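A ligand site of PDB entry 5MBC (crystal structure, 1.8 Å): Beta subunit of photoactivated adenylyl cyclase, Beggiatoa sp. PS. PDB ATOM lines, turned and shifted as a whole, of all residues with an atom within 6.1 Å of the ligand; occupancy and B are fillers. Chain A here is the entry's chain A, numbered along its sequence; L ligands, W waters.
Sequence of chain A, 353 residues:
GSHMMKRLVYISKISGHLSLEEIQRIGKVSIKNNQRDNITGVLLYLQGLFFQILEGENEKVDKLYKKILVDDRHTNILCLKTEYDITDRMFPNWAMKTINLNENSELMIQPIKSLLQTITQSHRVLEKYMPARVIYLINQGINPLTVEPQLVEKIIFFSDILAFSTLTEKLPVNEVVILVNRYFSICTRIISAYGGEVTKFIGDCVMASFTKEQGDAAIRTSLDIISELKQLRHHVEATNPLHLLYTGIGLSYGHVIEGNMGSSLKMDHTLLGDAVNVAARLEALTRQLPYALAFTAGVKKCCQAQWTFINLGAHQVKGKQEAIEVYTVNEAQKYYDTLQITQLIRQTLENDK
The side-chain amide nitrogen (ND2) of Asn 33 sits at hydrogen-bond distance from an oxygen (O1) of the ligand (3.0 Å). The side-chain amino group of Lys 67 lies within salt-bridge range of an oxygen (O7) of the ligand (3.7 Å). OD2 of Asp 71 lies within hydrogen-bond range of O3 of the ligand (2.7 Å). The side-chain amide nitrogen of Gln 52 is in hydrogen-bond range of a nitrogen (N3) of the ligand, 3.0 Å away. NH2 of Arg 73 sits at hydrogen-bond distance from O4 of the ligand, at 3.0 Å. The side-chain amide oxygen of Asn 34 is in hydrogen-bond range of a nitrogen (N2) of the ligand, at 2.9 Å.
NH2 of Arg 73 lies within salt-bridge range of OD2 of Asp 71. The side-chain sulfur (SD) of Met 96 sits at hydrogen-bond distance from the backbone NH (N) of Leu 43 (3.6 Å). The backbone carbonyl oxygen (O) of Asn 34 sits at hydrogen-bond distance from the backbone NH (N) of Ile 39 (2.6 Å). O of Ala 95 sits at hydrogen-bond distance from ND2 of Asn 34 (2.9 Å). A ring nitrogen (ND1) of His 74 is in hydrogen-bond range of the side-chain hydroxyl of Ser 12 (2.8 Å). OE1 of Gln 52 is in hydrogen-bond range of OH of Tyr 10, at 2.5 Å. The side-chain amide nitrogen of Gln 52 lies close to the side-chain sulfur of Met 96 (3.6 Å). The side-chain hydroxyl (OG) of Ser 30 is in hydrogen-bond range of the backbone carbonyl oxygen (O) of Ile 26 (2.5 Å).
Residues that only touch the ligand: Tyr 10, Ile 26, Val 29, Ser 30, Phe 50, Leu 54, Leu 64, Ile 68, His 74 and Met 96. 16 residues have an atom within 4 Å of the ligand: Tyr 10, Ile 26, Val 29, Ser 30, Asn 33, Asn 34, Phe 50, Gln 52, Leu 54, Leu 64, Lys 67, Ile 68, Asp 71, Arg 73, His 74 and Met 96.
Water W1 bridges OD1 of Asn 34 and O1 of the ligand.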
ATOM      1  N   TYR A  10       7.868   8.632 -22.720  1.00  0.00           N
ATOM      2  CA  TYR A  10       6.889   7.566 -22.766  1.00  0.00           C
ATOM      3  C   TYR A  10       6.747   6.932 -21.390  1.00  0.00           C
ATOM      4  O   TYR A  10       7.624   7.058 -20.523  1.00  0.00           O
ATOM      5  CB  TYR A  10       7.253   6.487 -23.798  1.00  0.00           C
ATOM      6  CG  TYR A  10       8.385   5.560 -23.389  1.00  0.00           C
ATOM      7  CD1 TYR A  10       8.124   4.388 -22.694  1.00  0.00           C
ATOM      8  CD2 TYR A  10       9.704   5.849 -23.721  1.00  0.00           C
ATOM      9  CE1 TYR A  10       9.144   3.537 -22.314  1.00  0.00           C
ATOM     10  CE2 TYR A  10      10.733   4.996 -23.351  1.00  0.00           C
ATOM     11  CZ  TYR A  10      10.449   3.845 -22.653  1.00  0.00           C
ATOM     12  OH  TYR A  10      11.474   2.999 -22.281  1.00  0.00           O
ATOM     13  N   SER A  12       5.329   3.053 -19.620  1.00  0.00           N
ATOM     14  CA  SER A  12       5.079   1.663 -19.963  1.00  0.00           C
ATOM     15  C   SER A  12       4.839   0.863 -18.688  1.00  0.00           C
ATOM     16  O   SER A  12       5.167   1.305 -17.584  1.00  0.00           O
ATOM     17  CB  SER A  12       6.235   1.054 -20.763  1.00  0.00           C
ATOM     18  OG  SER A  12       7.413   0.972 -19.983  1.00  0.00           O
ATOM     19  N   LEU A  18      10.370  -7.637 -12.548  1.00  0.00           N
ATOM     20  CA  LEU A  18      11.784  -7.453 -12.867  1.00  0.00           C
ATOM     21  C   LEU A  18      12.560  -7.174 -11.584  1.00  0.00           C
ATOM     22  O   LEU A  18      12.255  -6.216 -10.860  1.00  0.00           O
ATOM     23  CB  LEU A  18      11.978  -6.294 -13.844  1.00  0.00           C
ATOM     24  CG  LEU A  18      11.436  -6.441 -15.273  1.00  0.00           C
ATOM     25  CD1 LEU A  18      11.724  -5.213 -16.167  1.00  0.00           C
ATOM     26  CD2 LEU A  18      11.992  -7.708 -15.902  1.00  0.00           C
ATOM     27  N   ILE A  26      19.479  -3.078 -17.663  1.00  0.00           N
ATOM     28  CA  ILE A  26      18.981  -2.096 -18.613  1.00  0.00           C
ATOM     29  C   ILE A  26      19.796  -0.815 -18.525  1.00  0.00           C
ATOM     30  O   ILE A  26      20.187  -0.237 -19.549  1.00  0.00           O
ATOM     31  CB  ILE A  26      17.484  -1.808 -18.361  1.00  0.00           C
ATOM     32  CG1 ILE A  26      16.667  -3.091 -18.479  1.00  0.00           C
ATOM     33  CG2 ILE A  26      16.973  -0.751 -19.331  1.00  0.00           C
ATOM     34  CD1 ILE A  26      15.196  -2.904 -18.178  1.00  0.00           C
ATOM     35  N   VAL A  29      23.534  -1.321 -20.354  1.00  0.00           N
ATOM     36  CA  VAL A  29      23.517  -1.338 -21.809  1.00  0.00           C
ATOM     37  C   VAL A  29      22.974  -0.017 -22.369  1.00  0.00           C
ATOM     38  O   VAL A  29      23.364   0.400 -23.468  1.00  0.00           O
ATOM     39  CB  VAL A  29      22.702  -2.546 -22.324  1.00  0.00           C
ATOM     40  CG1 VAL A  29      21.248  -2.444 -21.902  1.00  0.00           C
ATOM     41  CG2 VAL A  29      22.826  -2.688 -23.835  1.00  0.00           C
ATOM     42  N   SER A  30      22.090   0.653 -21.627  1.00  0.00           N
ATOM     43  CA  SER A  30      21.606   1.954 -22.065  1.00  0.00           C
ATOM     44  C   SER A  30      22.716   2.994 -22.023  1.00  0.00           C
ATOM     45  O   SER A  30      22.876   3.778 -22.965  1.00  0.00           O
ATOM     46  CB  SER A  30      20.426   2.399 -21.207  1.00  0.00           C
ATOM     47  OG  SER A  30      19.403   1.408 -21.196  1.00  0.00           O
ATOM     48  N   ILE A  31      23.493   3.010 -20.939  1.00  0.00           N
ATOM     49  CA  ILE A  31      24.554   4.005 -20.796  1.00  0.00           C
ATOM     50  C   ILE A  31      25.580   3.869 -21.910  1.00  0.00           C
ATOM     51  O   ILE A  31      26.031   4.860 -22.491  1.00  0.00           O
ATOM     52  CB  ILE A  31      25.203   3.896 -19.401  1.00  0.00           C
ATOM     53  CG1 ILE A  31      24.285   4.472 -18.331  1.00  0.00           C
ATOM     54  CG2 ILE A  31      26.551   4.610 -19.377  1.00  0.00           C
ATOM     55  CD1 ILE A  31      24.779   4.278 -16.916  1.00  0.00           C
ATOM     56  N   ASN A  33      25.222   2.340 -24.982  1.00  0.00           N
ATOM     57  CA  ASN A  33      24.655   2.622 -26.292  1.00  0.00           C
ATOM     58  C   ASN A  33      24.337   4.103 -26.452  1.00  0.00           C
ATOM     59  O   ASN A  33      24.581   4.685 -27.508  1.00  0.00           O
ATOM     60  CB  ASN A  33      23.411   1.779 -26.527  1.00  0.00           C
ATOM     61  CG  ASN A  33      23.703   0.296 -26.608  1.00  0.00           C
ATOM     62  OD1 ASN A  33      24.849  -0.110 -26.791  1.00  0.00           O
ATOM     63  ND2 ASN A  33      22.669  -0.528 -26.457  1.00  0.00           N
ATOM     64  N   ASN A  34      23.785   4.726 -25.401  1.00  0.00           N
ATOM     65  CA  ASN A  34      23.450   6.146 -25.493  1.00  0.00           C
ATOM     66  C   ASN A  34      24.690   7.016 -25.572  1.00  0.00           C
ATOM     67  O   ASN A  34      24.668   8.064 -26.233  1.00  0.00           O
ATOM     68  CB  ASN A  34      22.588   6.560 -24.297  1.00  0.00           C
ATOM     69  CG  ASN A  34      21.217   5.891 -24.314  1.00  0.00           C
ATOM     70  OD1 ASN A  34      20.971   4.982 -25.097  1.00  0.00           O
ATOM     71  ND2 ASN A  34      20.333   6.332 -23.429  1.00  0.00           N
ATOM     72  N   ARG A  36      27.366   6.042 -27.146  1.00  0.00           N
ATOM     73  CA  ARG A  36      27.757   5.856 -28.539  1.00  0.00           C
ATOM     74  C   ARG A  36      26.930   6.727 -29.470  1.00  0.00           C
ATOM     75  O   ARG A  36      27.463   7.348 -30.391  1.00  0.00           O
ATOM     76  CB  ARG A  36      27.627   4.379 -28.910  1.00  0.00           C
ATOM     77  CG  ARG A  36      27.753   4.080 -30.399  1.00  0.00           C
ATOM     78  CD  ARG A  36      27.053   2.770 -30.741  1.00  0.00           C
ATOM     79  NE  ARG A  36      25.604   2.890 -30.624  1.00  0.00           N
ATOM     80  CZ  ARG A  36      24.769   1.862 -30.517  1.00  0.00           C
ATOM     81  NH1 ARG A  36      25.249   0.628 -30.498  1.00  0.00           N
ATOM     82  NH2 ARG A  36      23.468   2.063 -30.425  1.00  0.00           N
ATOM     83  N   ILE A  39      23.081   9.997 -27.010  1.00  0.00           N
ATOM     84  CA  ILE A  39      21.727  10.082 -26.470  1.00  0.00           C
ATOM     85  C   ILE A  39      21.810  10.275 -24.963  1.00  0.00           C
ATOM     86  O   ILE A  39      22.652   9.661 -24.294  1.00  0.00           O
ATOM     87  CB  ILE A  39      20.910   8.825 -26.822  1.00  0.00           C
ATOM     88  CG1 ILE A  39      20.645   8.764 -28.327  1.00  0.00           C
ATOM     89  CG2 ILE A  39      19.592   8.784 -26.048  1.00  0.00           C
ATOM     90  CD1 ILE A  39      19.811   7.575 -28.759  1.00  0.00           C
ATOM     91  N   LEU A  43      15.603   7.412 -16.745  1.00  0.00           N
ATOM     92  CA  LEU A  43      14.677   6.289 -16.645  1.00  0.00           C
ATOM     93  C   LEU A  43      14.193   6.172 -15.209  1.00  0.00           C
ATOM     94  O   LEU A  43      14.996   5.907 -14.298  1.00  0.00           O
ATOM     95  CB  LEU A  43      15.333   4.982 -17.093  1.00  0.00           C
ATOM     96  CG  LEU A  43      14.481   3.716 -16.951  1.00  0.00           C
ATOM     97  CD1 LEU A  43      13.208   3.813 -17.769  1.00  0.00           C
ATOM     98  CD2 LEU A  43      15.274   2.475 -17.335  1.00  0.00           C
ATOM     99  N   PHE A  50       7.183   2.160 -15.899  1.00  0.00           N
ATOM    100  CA  PHE A  50       8.421   2.766 -16.379  1.00  0.00           C
ATOM    101  C   PHE A  50       8.153   4.182 -16.879  1.00  0.00           C
ATOM    102  O   PHE A  50       7.140   4.438 -17.530  1.00  0.00           O
ATOM    103  CB  PHE A  50       9.054   1.944 -17.490  1.00  0.00           C
ATOM    104  CG  PHE A  50       9.909   0.794 -17.009  1.00  0.00           C
ATOM    105  CD1 PHE A  50      10.778   0.969 -15.951  1.00  0.00           C
ATOM    106  CD2 PHE A  50       9.831  -0.448 -17.611  1.00  0.00           C
ATOM    107  CE1 PHE A  50      11.569  -0.085 -15.500  1.00  0.00           C
ATOM    108  CE2 PHE A  50      10.610  -1.502 -17.179  1.00  0.00           C
ATOM    109  CZ  PHE A  50      11.483  -1.316 -16.113  1.00  0.00           C
ATOM    110  N   GLN A  52      10.470   7.110 -18.985  1.00  0.00           N
ATOM    111  CA  GLN A  52      11.750   7.378 -19.631  1.00  0.00           C
ATOM    112  C   GLN A  52      11.655   8.604 -20.521  1.00  0.00           C
ATOM    113  O   GLN A  52      10.683   8.772 -21.269  1.00  0.00           O
ATOM    114  CB  GLN A  52      12.242   6.176 -20.446  1.00  0.00           C
ATOM    115  CG  GLN A  52      13.670   6.343 -20.928  1.00  0.00           C
ATOM    116  CD  GLN A  52      14.254   5.061 -21.501  1.00  0.00           C
ATOM    117  OE1 GLN A  52      13.572   4.327 -22.210  1.00  0.00           O
ATOM    118  NE2 GLN A  52      15.519   4.798 -21.190  1.00  0.00           N
ATOM    119  N   LEU A  54      14.001  10.506 -23.488  1.00  0.00           N
ATOM    120  CA  LEU A  54      15.110  10.292 -24.416  1.00  0.00           C
ATOM    121  C   LEU A  54      15.302  11.546 -25.248  1.00  0.00           C
ATOM    122  O   LEU A  54      14.321  12.170 -25.689  1.00  0.00           O
ATOM    123  CB  LEU A  54      14.850   9.083 -25.326  1.00  0.00           C
ATOM    124  CG  LEU A  54      14.788   7.713 -24.658  1.00  0.00           C
ATOM    125  CD1 LEU A  54      14.216   6.684 -25.626  1.00  0.00           C
ATOM    126  CD2 LEU A  54      16.168   7.286 -24.179  1.00  0.00           C
ATOM    127  N   LEU A  64      16.505   4.063 -31.578  1.00  0.00           N
ATOM    128  CA  LEU A  64      16.473   3.459 -30.257  1.00  0.00           C
ATOM    129  C   LEU A  64      15.037   3.145 -29.830  1.00  0.00           C
ATOM    130  O   LEU A  64      14.792   2.109 -29.203  1.00  0.00           O
ATOM    131  CB  LEU A  64      17.133   4.388 -29.236  1.00  0.00           C
ATOM    132  CG  LEU A  64      17.032   3.984 -27.769  1.00  0.00           C
ATOM    133  CD1 LEU A  64      17.619   2.605 -27.546  1.00  0.00           C
ATOM    134  CD2 LEU A  64      17.719   5.019 -26.884  1.00  0.00           C
ATOM    135  N   LYS A  67      13.633  -0.085 -31.071  1.00  0.00           N
ATOM    136  CA  LYS A  67      14.178  -1.228 -30.344  1.00  0.00           C
ATOM    137  C   LYS A  67      13.567  -1.337 -28.952  1.00  0.00           C
ATOM    138  O   LYS A  67      13.325  -2.443 -28.467  1.00  0.00           O
ATOM    139  CB  LYS A  67      15.696  -1.111 -30.271  1.00  0.00           C
ATOM    140  CG  LYS A  67      16.382  -2.258 -29.555  1.00  0.00           C
ATOM    141  CD  LYS A  67      17.895  -2.152 -29.692  1.00  0.00           C
ATOM    142  CE  LYS A  67      18.394  -0.761 -29.315  1.00  0.00           C
ATOM    143  NZ  LYS A  67      19.884  -0.674 -29.345  1.00  0.00           N
ATOM    144  N   ILE A  68      13.305  -0.197 -28.304  1.00  0.00           N
ATOM    145  CA  ILE A  68      12.663  -0.218 -26.999  1.00  0.00           C
ATOM    146  C   ILE A  68      11.227  -0.718 -27.115  1.00  0.00           C
ATOM    147  O   ILE A  68      10.708  -1.357 -26.186  1.00  0.00           O
ATOM    148  CB  ILE A  68      12.731   1.192 -26.362  1.00  0.00           C
ATOM    149  CG1 ILE A  68      14.181   1.581 -26.092  1.00  0.00           C
ATOM    150  CG2 ILE A  68      11.941   1.242 -25.069  1.00  0.00           C
ATOM    151  CD1 ILE A  68      14.342   2.921 -25.405  1.00  0.00           C
ATOM    152  N   LEU A  69      10.564  -0.463 -28.253  1.00  0.00           N
ATOM    153  CA  LEU A  69       9.184  -0.893 -28.424  1.00  0.00           C
ATOM    154  C   LEU A  69       9.053  -2.404 -28.368  1.00  0.00           C
ATOM    155  O   LEU A  69       8.094  -2.939 -27.788  1.00  0.00           O
ATOM    156  CB  LEU A  69       8.623  -0.365 -29.742  1.00  0.00           C
ATOM    157  CG  LEU A  69       8.118   1.085 -29.779  1.00  0.00           C
ATOM    158  CD1 LEU A  69       7.589   1.420 -31.165  1.00  0.00           C
ATOM    159  CD2 LEU A  69       7.057   1.319 -28.719  1.00  0.00           C
ATOM    160  N   ASP A  71      10.922  -4.510 -26.868  1.00  0.00           N
ATOM    161  CA  ASP A  71      11.620  -5.082 -25.724  1.00  0.00           C
ATOM    162  C   ASP A  71      10.678  -5.976 -24.926  1.00  0.00           C
ATOM    163  O   ASP A  71       9.494  -5.666 -24.750  1.00  0.00           O
ATOM    164  CB  ASP A  71      12.183  -3.982 -24.830  1.00  0.00           C
ATOM    165  CG  ASP A  71      13.206  -4.493 -23.848  1.00  0.00           C
ATOM    166  OD1 ASP A  71      12.820  -5.132 -22.853  1.00  0.00           O
ATOM    167  OD2 ASP A  71      14.419  -4.252 -24.070  1.00  0.00           O
ATOM    168  N   ARG A  73      10.749  -6.586 -21.739  1.00  0.00           N
ATOM    169  CA  ARG A  73      10.656  -6.263 -20.322  1.00  0.00           C
ATOM    170  C   ARG A  73       9.601  -5.215 -19.982  1.00  0.00           C
ATOM    171  O   ARG A  73       9.482  -4.843 -18.810  1.00  0.00           O
ATOM    172  CB  ARG A  73      12.025  -5.807 -19.807  1.00  0.00           C
ATOM    173  CG  ARG A  73      13.044  -6.938 -19.719  1.00  0.00           C
ATOM    174  CD  ARG A  73      14.475  -6.431 -19.667  1.00  0.00           C
ATOM    175  NE  ARG A  73      14.909  -5.897 -20.966  1.00  0.00           N
ATOM    176  CZ  ARG A  73      16.162  -5.592 -21.253  1.00  0.00           C
ATOM    177  NH1 ARG A  73      17.119  -5.767 -20.347  1.00  0.00           N
ATOM    178  NH2 ARG A  73      16.475  -5.112 -22.453  1.00  0.00           N
ATOM    179  N   HIS A  74       8.828  -4.734 -20.950  1.00  0.00           N
ATOM    180  CA  HIS A  74       7.733  -3.823 -20.648  1.00  0.00           C
ATOM    181  C   HIS A  74       6.673  -3.910 -21.740  1.00  0.00           C
ATOM    182  O   HIS A  74       6.959  -4.312 -22.875  1.00  0.00           O
ATOM    183  CB  HIS A  74       8.219  -2.381 -20.466  1.00  0.00           C
ATOM    184  CG  HIS A  74       8.861  -1.790 -21.685  1.00  0.00           C
ATOM    185  ND1 HIS A  74       9.072  -0.433 -21.823  1.00  0.00           N
ATOM    186  CD2 HIS A  74       9.328  -2.361 -22.821  1.00  0.00           C
ATOM    187  CE1 HIS A  74       9.653  -0.201 -22.995  1.00  0.00           C
ATOM    188  NE2 HIS A  74       9.816  -1.355 -23.611  1.00  0.00           N
ATOM    189  N   ALA A  95      23.916   9.964 -19.746  1.00  0.00           N
ATOM    190  CA  ALA A  95      23.650   9.085 -20.876  1.00  0.00           C
ATOM    191  C   ALA A  95      22.356   8.306 -20.667  1.00  0.00           C
ATOM    192  O   ALA A  95      21.511   8.202 -21.568  1.00  0.00           O
ATOM    193  CB  ALA A  95      24.824   8.131 -21.089  1.00  0.00           C
ATOM    194  N   MET A  96      22.179   7.761 -19.458  1.00  0.00           N
ATOM    195  CA  MET A  96      20.879   7.216 -19.046  1.00  0.00           C
ATOM    196  C   MET A  96      20.910   7.092 -17.525  1.00  0.00           C
ATOM    197  O   MET A  96      21.502   6.151 -16.989  1.00  0.00           O
ATOM    198  CB  MET A  96      20.589   5.880 -19.703  1.00  0.00           C
ATOM    199  CG  MET A  96      19.228   5.312 -19.338  1.00  0.00           C
ATOM    200  SD  MET A  96      17.943   6.572 -19.297  1.00  0.00           S
ATOM    201  CE  MET A  96      17.908   7.103 -21.008  1.00  0.00           C
HETATM  202  N1  LIG L   1      18.647   0.499 -24.509  1.00  0.00           N
HETATM  203  C1  LIG L   1      19.446   1.549 -24.871  1.00  0.00           C
HETATM  204  O1  LIG L   1      20.436   1.351 -25.583  1.00  0.00           O
HETATM  205  N2  LIG L   1      19.157   2.828 -24.442  1.00  0.00           N
HETATM  206  C2  LIG L   1      18.053   3.044 -23.642  1.00  0.00           C
HETATM  207  O2  LIG L   1      17.796   4.185 -23.256  1.00  0.00           O
HETATM  208  C3  LIG L   1      17.243   1.986 -23.278  1.00  0.00           C
HETATM  209  N3  LIG L   1      16.139   2.202 -22.478  1.00  0.00           N
HETATM  210  C4  LIG L   1      15.324   1.152 -22.111  1.00  0.00           C
HETATM  211  C5  LIG L   1      14.223   1.379 -21.302  1.00  0.00           C
HETATM  212  C6  LIG L   1      13.399   0.326 -20.942  1.00  0.00           C
HETATM  213  C7  LIG L   1      12.202   0.579 -20.071  1.00  0.00           C
HETATM  214  C8  LIG L   1      13.694  -0.962 -21.374  1.00  0.00           C
HETATM  215  C9  LIG L   1      12.806  -2.111 -20.968  1.00  0.00           C
HETATM  216  C10 LIG L   1      14.804  -1.199 -22.172  1.00  0.00           C
HETATM  217  C11 LIG L   1      15.627  -0.138 -22.554  1.00  0.00           C
HETATM  218  N4  LIG L   1      16.727  -0.359 -23.347  1.00  0.00           N
HETATM  219  C12 LIG L   1      17.537   0.699 -23.710  1.00  0.00           C
HETATM  220  C13 LIG L   1      17.041  -1.756 -23.820  1.00  0.00           C
HETATM  221  C14 LIG L   1      16.763  -1.919 -25.311  1.00  0.00           C
HETATM  222  O3  LIG L   1      15.393  -2.151 -25.521  1.00  0.00           O
HETATM  223  C15 LIG L   1      17.568  -3.081 -25.885  1.00  0.00           C
HETATM  224  O4  LIG L   1      17.226  -4.265 -25.200  1.00  0.00           O
HETATM  225  C16 LIG L   1      19.072  -2.845 -25.749  1.00  0.00           C
HETATM  226  O5  LIG L   1      19.435  -1.669 -26.442  1.00  0.00           O
HETATM  227  C17 LIG L   1      19.839  -4.036 -26.311  1.00  0.00           C
HETATM  228  O6  LIG L   1      20.467  -3.708 -27.524  1.00  0.00           O
HETATM  229  P1  LIG L   1      20.661  -4.838 -28.652  1.00  0.00           P
HETATM  230  O7  LIG L   1      20.285  -4.255 -29.996  1.00  0.00           O
HETATM  231  O8  LIG L   1      22.102  -5.296 -28.682  1.00  0.00           O
HETATM  232  O9  LIG L   1      19.764  -6.007 -28.344  1.00  0.00           O
HETATM  233  O   HOH W   1      21.023   3.772 -28.000  1.00  0.00           O
